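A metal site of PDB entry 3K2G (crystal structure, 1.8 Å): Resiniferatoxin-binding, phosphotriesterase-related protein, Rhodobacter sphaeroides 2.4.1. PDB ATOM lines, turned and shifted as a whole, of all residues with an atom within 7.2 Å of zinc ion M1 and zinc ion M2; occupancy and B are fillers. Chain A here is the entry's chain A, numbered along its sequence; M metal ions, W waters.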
ATOM      1  N   HIS A  34     -12.072   4.074  10.232  1.00  0.00           N
ATOM      2  CA  HIS A  34     -12.751   4.300  11.504  1.00  0.00           C
ATOM      3  C   HIS A  34     -14.202   4.737  11.312  1.00  0.00           C
ATOM      4  O   HIS A  34     -14.483   5.917  11.108  1.00  0.00           O
ATOM      5  CB  HIS A  34     -11.958   5.370  12.285  1.00  0.00           C
ATOM      6  CG  HIS A  34     -12.467   5.638  13.673  1.00  0.00           C
ATOM      7  ND1 HIS A  34     -11.646   5.634  14.777  1.00  0.00           N
ATOM      8  CD2 HIS A  34     -13.704   5.923  14.129  1.00  0.00           C
ATOM      9  CE1 HIS A  34     -12.348   5.900  15.857  1.00  0.00           C
ATOM     10  NE2 HIS A  34     -13.606   6.089  15.492  1.00  0.00           N
ATOM     11  N   GLU A  35     -15.111   3.762  11.377  1.00  0.00           N
ATOM     12  CA  GLU A  35     -16.545   4.011  11.224  1.00  0.00           C
ATOM     13  C   GLU A  35     -17.318   3.111  12.184  1.00  0.00           C
ATOM     14  O   GLU A  35     -16.875   2.004  12.499  1.00  0.00           O
ATOM     15  CB  GLU A  35     -17.006   3.686   9.792  1.00  0.00           C
ATOM     16  CG  GLU A  35     -16.231   4.359   8.665  1.00  0.00           C
ATOM     17  CD  GLU A  35     -16.333   5.870   8.698  1.00  0.00           C
ATOM     18  OE1 GLU A  35     -17.302   6.397   9.288  1.00  0.00           O
ATOM     19  OE2 GLU A  35     -15.455   6.533   8.118  1.00  0.00           O
ATOM     20  N   HIS A  36     -18.467   3.586  12.640  1.00  0.00           N
ATOM     21  CA  HIS A  36     -19.316   2.781  13.526  1.00  0.00           C
ATOM     22  C   HIS A  36     -20.541   2.385  12.708  1.00  0.00           C
ATOM     23  O   HIS A  36     -21.244   3.245  12.177  1.00  0.00           O
ATOM     24  CB  HIS A  36     -19.701   3.586  14.753  1.00  0.00           C
ATOM     25  CG  HIS A  36     -18.546   3.944  15.628  1.00  0.00           C
ATOM     26  ND1 HIS A  36     -17.963   3.044  16.500  1.00  0.00           N
ATOM     27  CD2 HIS A  36     -17.808   5.084  15.721  1.00  0.00           C
ATOM     28  CE1 HIS A  36     -16.927   3.621  17.094  1.00  0.00           C
ATOM     29  NE2 HIS A  36     -16.811   4.852  16.629  1.00  0.00           N
ATOM     30  N   ASN A  39     -23.951   0.957  17.151  1.00  0.00           N
ATOM     31  CA  ASN A  39     -23.395   1.357  18.423  1.00  0.00           C
ATOM     32  C   ASN A  39     -24.456   1.865  19.377  1.00  0.00           C
ATOM     33  O   ASN A  39     -25.640   1.961  19.034  1.00  0.00           O
ATOM     34  CB  ASN A  39     -22.299   2.422  18.225  1.00  0.00           C
ATOM     35  CG  ASN A  39     -22.853   3.803  17.895  1.00  0.00           C
ATOM     36  OD1 ASN A  39     -24.061   3.968  17.725  1.00  0.00           O
ATOM     37  ND2 ASN A  39     -21.965   4.787  17.820  1.00  0.00           N
ATOM     38  N   PRO A 106     -14.223   0.220  14.928  1.00  0.00           N
ATOM     39  CA  PRO A 106     -13.593   0.183  16.246  1.00  0.00           C
ATOM     40  C   PRO A 106     -14.532   0.218  17.443  1.00  0.00           C
ATOM     41  O   PRO A 106     -14.101   0.503  18.558  1.00  0.00           O
ATOM     42  CB  PRO A 106     -12.656   1.370  16.193  1.00  0.00           C
ATOM     43  CG  PRO A 106     -13.453   2.379  15.456  1.00  0.00           C
ATOM     44  CD  PRO A 106     -14.168   1.590  14.368  1.00  0.00           C
ATOM     45  N   THR A 107     -15.818  -0.058  17.223  1.00  0.00           N
ATOM     46  CA  THR A 107     -16.771  -0.058  18.327  1.00  0.00           C
ATOM     47  C   THR A 107     -16.327  -1.168  19.280  1.00  0.00           C
ATOM     48  O   THR A 107     -16.242  -2.322  18.893  1.00  0.00           O
ATOM     49  CB  THR A 107     -18.195  -0.391  17.836  1.00  0.00           C
ATOM     50  OG1 THR A 107     -18.574   0.494  16.780  1.00  0.00           O
ATOM     51  CG2 THR A 107     -19.196  -0.262  18.968  1.00  0.00           C
ATOM     52  N   ILE A 111     -19.725   0.370  24.190  1.00  0.00           N
ATOM     53  CA  ILE A 111     -20.453   1.146  23.197  1.00  0.00           C
ATOM     54  C   ILE A 111     -21.217   0.330  22.141  1.00  0.00           C
ATOM     55  O   ILE A 111     -21.526   0.839  21.066  1.00  0.00           O
ATOM     56  CB  ILE A 111     -19.547   2.208  22.506  1.00  0.00           C
ATOM     57  CG1 ILE A 111     -18.240   1.578  22.014  1.00  0.00           C
ATOM     58  CG2 ILE A 111     -19.259   3.349  23.462  1.00  0.00           C
ATOM     59  CD1 ILE A 111     -17.357   2.556  21.262  1.00  0.00           C
ATOM     60  N   TYR A 136     -13.553   1.479  26.221  1.00  0.00           N
ATOM     61  CA  TYR A 136     -13.632   2.864  25.786  1.00  0.00           C
ATOM     62  C   TYR A 136     -13.472   3.835  26.967  1.00  0.00           C
ATOM     63  O   TYR A 136     -12.819   3.513  27.953  1.00  0.00           O
ATOM     64  CB  TYR A 136     -14.969   3.083  25.073  1.00  0.00           C
ATOM     65  CG  TYR A 136     -14.998   4.275  24.159  1.00  0.00           C
ATOM     66  CD1 TYR A 136     -13.943   4.532  23.287  1.00  0.00           C
ATOM     67  CD2 TYR A 136     -16.098   5.118  24.119  1.00  0.00           C
ATOM     68  CE1 TYR A 136     -13.992   5.606  22.391  1.00  0.00           C
ATOM     69  CE2 TYR A 136     -16.163   6.184  23.236  1.00  0.00           C
ATOM     70  CZ  TYR A 136     -15.109   6.429  22.377  1.00  0.00           C
ATOM     71  OH  TYR A 136     -15.181   7.464  21.481  1.00  0.00           O
ATOM     72  N   LEU A 137     -14.059   5.022  26.847  1.00  0.00           N
ATOM     73  CA  LEU A 137     -13.969   6.037  27.904  1.00  0.00           C
ATOM     74  C   LEU A 137     -14.548   5.556  29.235  1.00  0.00           C
ATOM     75  O   LEU A 137     -15.476   4.756  29.264  1.00  0.00           O
ATOM     76  CB  LEU A 137     -14.662   7.322  27.445  1.00  0.00           C
ATOM     77  CG  LEU A 137     -14.044   7.949  26.201  1.00  0.00           C
ATOM     78  CD1 LEU A 137     -14.933   9.065  25.697  1.00  0.00           C
ATOM     79  CD2 LEU A 137     -12.641   8.483  26.517  1.00  0.00           C
ATOM     80  N   GLU A 177      -9.875   1.652  19.623  1.00  0.00           N
ATOM     81  CA  GLU A 177     -10.680   2.826  19.807  1.00  0.00           C
ATOM     82  C   GLU A 177     -10.648   2.670  21.319  1.00  0.00           C
ATOM     83  O   GLU A 177     -11.698   2.528  21.960  1.00  0.00           O
ATOM     84  CB  GLU A 177     -12.098   2.692  19.252  1.00  0.00           C
ATOM     85  CG  GLU A 177     -13.084   3.701  19.852  1.00  0.00           C
ATOM     86  CD  GLU A 177     -13.349   5.000  19.075  1.00  0.00           C
ATOM     87  OE1 GLU A 177     -12.599   5.988  19.231  1.00  0.00           O
ATOM     88  OE2 GLU A 177     -14.367   5.038  18.335  1.00  0.00           O
ATOM     89  N   ILE A 178      -9.438   2.659  21.888  1.00  0.00           N
ATOM     90  CA  ILE A 178      -9.254   2.520  23.328  1.00  0.00           C
ATOM     91  C   ILE A 178      -9.481   3.919  23.894  1.00  0.00           C
ATOM     92  O   ILE A 178      -8.899   4.883  23.394  1.00  0.00           O
ATOM     93  CB  ILE A 178      -7.821   2.024  23.689  1.00  0.00           C
ATOM     94  CG1 ILE A 178      -7.570   0.645  23.075  1.00  0.00           C
ATOM     95  CG2 ILE A 178      -7.636   1.957  25.217  1.00  0.00           C
ATOM     96  CD1 ILE A 178      -8.567  -0.403  23.526  1.00  0.00           C
ATOM     97  N   GLY A 179     -10.313   4.022  24.921  1.00  0.00           N
ATOM     98  CA  GLY A 179     -10.637   5.321  25.478  1.00  0.00           C
ATOM     99  C   GLY A 179      -9.693   6.075  26.383  1.00  0.00           C
ATOM    100  O   GLY A 179      -9.359   5.635  27.481  1.00  0.00           O
ATOM    101  N   MET A 207      -5.333   1.064  18.065  1.00  0.00           N
ATOM    102  CA  MET A 207      -5.989   2.321  17.741  1.00  0.00           C
ATOM    103  C   MET A 207      -6.448   2.980  19.038  1.00  0.00           C
ATOM    104  O   MET A 207      -7.157   2.362  19.837  1.00  0.00           O
ATOM    105  CB  MET A 207      -7.196   2.057  16.841  1.00  0.00           C
ATOM    106  CG  MET A 207      -7.955   3.312  16.385  1.00  0.00           C
ATOM    107  SD  MET A 207      -9.411   2.852  15.246  1.00  0.00           S
ATOM    108  CE  MET A 207      -8.418   2.598  13.617  1.00  0.00           C
ATOM    109  N   VAL A 208      -6.043   4.221  19.249  1.00  0.00           N
ATOM    110  CA  VAL A 208      -6.410   4.918  20.477  1.00  0.00           C
ATOM    111  C   VAL A 208      -7.248   6.170  20.278  1.00  0.00           C
ATOM    112  O   VAL A 208      -6.927   7.056  19.494  1.00  0.00           O
ATOM    113  CB  VAL A 208      -5.134   5.319  21.268  1.00  0.00           C
ATOM    114  CG1 VAL A 208      -5.531   5.815  22.655  1.00  0.00           C
ATOM    115  CG2 VAL A 208      -4.197   4.130  21.391  1.00  0.00           C
ATOM    116  N   HIS A 209      -8.353   6.234  21.014  1.00  0.00           N
ATOM    117  CA  HIS A 209      -9.225   7.402  20.960  1.00  0.00           C
ATOM    118  C   HIS A 209      -8.535   8.501  21.736  1.00  0.00           C
ATOM    119  O   HIS A 209      -8.095   8.290  22.865  1.00  0.00           O
ATOM    120  CB  HIS A 209     -10.570   7.110  21.635  1.00  0.00           C
ATOM    121  CG  HIS A 209     -11.295   8.338  22.087  1.00  0.00           C
ATOM    122  ND1 HIS A 209     -12.404   8.834  21.433  1.00  0.00           N
ATOM    123  CD2 HIS A 209     -11.081   9.169  23.139  1.00  0.00           C
ATOM    124  CE1 HIS A 209     -12.840   9.914  22.060  1.00  0.00           C
ATOM    125  NE2 HIS A 209     -12.056  10.140  23.098  1.00  0.00           N
ATOM    126  N   LEU A 210      -8.441   9.676  21.142  1.00  0.00           N
ATOM    127  CA  LEU A 210      -7.805  10.785  21.819  1.00  0.00           C
ATOM    128  C   LEU A 210      -8.804  11.906  22.006  1.00  0.00           C
ATOM    129  O   LEU A 210      -9.750  12.045  21.226  1.00  0.00           O
ATOM    130  CB  LEU A 210      -6.635  11.329  21.006  1.00  0.00           C
ATOM    131  CG  LEU A 210      -5.382  10.481  20.825  1.00  0.00           C
ATOM    132  CD1 LEU A 210      -4.472  11.148  19.797  1.00  0.00           C
ATOM    133  CD2 LEU A 210      -4.666  10.344  22.144  1.00  0.00           C
ATOM    134  N   CYS A 237      -6.388   8.397  16.911  1.00  0.00           N
ATOM    135  CA  CYS A 237      -7.653   8.880  16.369  1.00  0.00           C
ATOM    136  C   CYS A 237      -7.902  10.355  16.643  1.00  0.00           C
ATOM    137  O   CYS A 237      -7.206  10.981  17.439  1.00  0.00           O
ATOM    138  CB  CYS A 237      -8.833   8.106  16.956  1.00  0.00           C
ATOM    139  SG  CYS A 237      -8.748   6.335  16.692  1.00  0.00           S
ATOM    140  N   HIS A 238      -8.897  10.909  15.964  1.00  0.00           N
ATOM    141  CA  HIS A 238      -9.326  12.289  16.145  1.00  0.00           C
ATOM    142  C   HIS A 238      -8.275  13.397  16.118  1.00  0.00           C
ATOM    143  O   HIS A 238      -8.227  14.242  17.010  1.00  0.00           O
ATOM    144  CB  HIS A 238     -10.138  12.347  17.436  1.00  0.00           C
ATOM    145  CG  HIS A 238     -11.041  11.179  17.625  1.00  0.00           C
ATOM    146  ND1 HIS A 238     -11.763  10.631  16.578  1.00  0.00           N
ATOM    147  CD2 HIS A 238     -11.334  10.427  18.715  1.00  0.00           C
ATOM    148  CE1 HIS A 238     -12.453   9.589  17.024  1.00  0.00           C
ATOM    149  NE2 HIS A 238     -12.207   9.444  18.315  1.00  0.00           N
ATOM    150  N   GLU A 260      -4.756   9.840  12.383  1.00  0.00           N
ATOM    151  CA  GLU A 260      -6.049   9.599  11.776  1.00  0.00           C
ATOM    152  C   GLU A 260      -7.020  10.779  11.833  1.00  0.00           C
ATOM    153  O   GLU A 260      -7.465  11.187  12.905  1.00  0.00           O
ATOM    154  CB  GLU A 260      -6.689   8.354  12.415  1.00  0.00           C
ATOM    155  CG  GLU A 260      -7.978   7.900  11.729  1.00  0.00           C
ATOM    156  CD  GLU A 260      -8.533   6.621  12.335  1.00  0.00           C
ATOM    157  OE1 GLU A 260      -9.230   6.705  13.372  1.00  0.00           O
ATOM    158  OE2 GLU A 260      -8.261   5.532  11.800  1.00  0.00           O
ATOM    159  N   ASP A 262     -10.184  11.179  11.252  1.00  0.00           N
ATOM    160  CA  ASP A 262     -11.433  10.440  11.149  1.00  0.00           C
ATOM    161  C   ASP A 262     -12.699  11.258  11.348  1.00  0.00           C
ATOM    162  O   ASP A 262     -13.765  10.686  11.580  1.00  0.00           O
ATOM    163  CB  ASP A 262     -11.411   9.283  12.169  1.00  0.00           C
ATOM    164  CG  ASP A 262     -10.844   9.713  13.516  1.00  0.00           C
ATOM    165  OD1 ASP A 262     -11.207  10.807  13.988  1.00  0.00           O
ATOM    166  OD2 ASP A 262     -10.038   8.940  14.099  1.00  0.00           O
ATOM    167  N   MET A 263     -12.606  12.577  11.258  1.00  0.00           N
ATOM    168  CA  MET A 263     -13.780  13.408  11.475  1.00  0.00           C
ATOM    169  C   MET A 263     -14.115  14.248  10.239  1.00  0.00           C
ATOM    170  O   MET A 263     -14.701  15.323  10.338  1.00  0.00           O
ATOM    171  CB  MET A 263     -13.544  14.291  12.698  1.00  0.00           C
ATOM    172  CG  MET A 263     -13.079  13.485  13.913  1.00  0.00           C
ATOM    173  SD  MET A 263     -12.448  14.579  15.417  1.00  0.00           S
ATOM    174  CE  MET A 263     -13.567  13.760  16.830  1.00  0.00           C
ATOM    175  N   ASP A 304     -15.914   8.713  11.123  1.00  0.00           N
ATOM    176  CA  ASP A 304     -16.285   8.423  12.513  1.00  0.00           C
ATOM    177  C   ASP A 304     -17.795   8.556  12.641  1.00  0.00           C
ATOM    178  O   ASP A 304     -18.310   9.162  13.575  1.00  0.00           O
ATOM    179  CB  ASP A 304     -15.590   9.323  13.549  1.00  0.00           C
ATOM    180  CG  ASP A 304     -15.763   8.808  14.987  1.00  0.00           C
ATOM    181  OD1 ASP A 304     -15.988   7.593  15.141  1.00  0.00           O
ATOM    182  OD2 ASP A 304     -15.673   9.595  15.959  1.00  0.00           O
ATOM    183  N   VAL A 305     -18.523   7.994  11.681  1.00  0.00           N
ATOM    184  CA  VAL A 305     -19.973   8.027  11.762  1.00  0.00           C
ATOM    185  C   VAL A 305     -20.291   7.355  13.095  1.00  0.00           C
ATOM    186  O   VAL A 305     -19.874   6.218  13.326  1.00  0.00           O
ATOM    187  CB  VAL A 305     -20.617   7.208  10.642  1.00  0.00           C
ATOM    188  CG1 VAL A 305     -22.108   7.058  10.880  1.00  0.00           C
ATOM    189  CG2 VAL A 305     -20.362   7.897   9.291  1.00  0.00           C
ATOM    190  N   PHE A 306     -21.011   8.062  13.979  1.00  0.00           N
ATOM    191  CA  PHE A 306     -21.354   7.450  15.261  1.00  0.00           C
ATOM    192  C   PHE A 306     -22.728   7.842  15.822  1.00  0.00           C
ATOM    193  O   PHE A 306     -23.098   7.413  16.913  1.00  0.00           O
ATOM    194  CB  PHE A 306     -20.248   7.716  16.295  1.00  0.00           C
ATOM    195  CG  PHE A 306     -20.323   9.058  16.949  1.00  0.00           C
ATOM    196  CD1 PHE A 306     -20.933   9.215  18.187  1.00  0.00           C
ATOM    197  CD2 PHE A 306     -19.771  10.177  16.327  1.00  0.00           C
ATOM    198  CE1 PHE A 306     -20.982  10.462  18.807  1.00  0.00           C
ATOM    199  CE2 PHE A 306     -19.812  11.426  16.935  1.00  0.00           C
ATOM    200  CZ  PHE A 306     -20.425  11.570  18.176  1.00  0.00           C
HETATM  201 ZN    ZN M   1     -13.585   7.991  19.575  1.00  0.00          ZN
HETATM  202 ZN    ZN M   2     -15.236   6.326  16.866  1.00  0.00          ZN
HETATM  203  O   HOH W   1     -15.200   9.685  20.004  1.00  0.00           O
HETATM  204  O   HOH W   2     -17.532   7.564  18.766  1.00  0.00           O
HETATM  205  O   HOH W   3     -15.190   8.002  18.124  1.00  0.00           O
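Of the 24 residues printed, 4 come within 4 Å of zinc ion M2. The nearest printed residue that does not touch zinc ion M2 is His 238 (4.3 Å).
Four residues have an atom within 4 Å of zinc ion M1: Tyr 136, Glu 177, His 209 and His 238. The nearest printed residue that does not touch zinc ion M1 is His 34 (4.4 Å).
ND1 of His 238 lies within hydrogen-bond range of OD1 of Asp 262, at 2.7 Å. N of His 209 sits at hydrogen-bond distance from O of Ile 178 (2.8 Å). The backbone NH (N) of Asp 304 sits at hydrogen-bond distance from the side-chain carboxylate (OE1) of Glu 35. ND1 of His 36 sits at hydrogen-bond distance from OG1 of Thr 107 (2.6 Å). ND1 of His 34 lies within hydrogen-bond range of SG of Cys 237 (3.5 Å). The backbone NH (N) of Glu 177 lies within hydrogen-bond range of the backbone carbonyl oxygen (O) of Met 207. SD of Met 207 sits at hydrogen-bond distance from ND1 of His 34 (3.6 Å). The backbone NH of His 238 lies within hydrogen-bond range of the backbone carbonyl oxygen of Glu 260 (3.4 Å).
Water W3 binds zinc ion M1, at 2.2 Å. Zinc ion M1 is bound by the side-chain carboxylate (OE1) of Glu 177, at 2.3 Å. A ring nitrogen (ND1) of His 209 is bound to zinc ion M1 (2.4 Å). NE2 of His 238 is bound to zinc ion M1, 2.4 Å away. Water W1 binds zinc ion M1 (2.4 Å). Zinc ion M1 is bound by OH of Tyr 136 (2.5 Å). Zinc ion M1 has six donor atoms within binding distance.
Zinc ion M2 is bound by water W3 (2.1 Å), the side-chain carboxylate of Glu 177 (2.1 Å), a ring nitrogen (NE2) of His 34 (2.1 Å), a ring nitrogen (NE2) of His 36 (2.2 Å) and the side-chain carboxylate of Asp 304 (2.3 Å).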
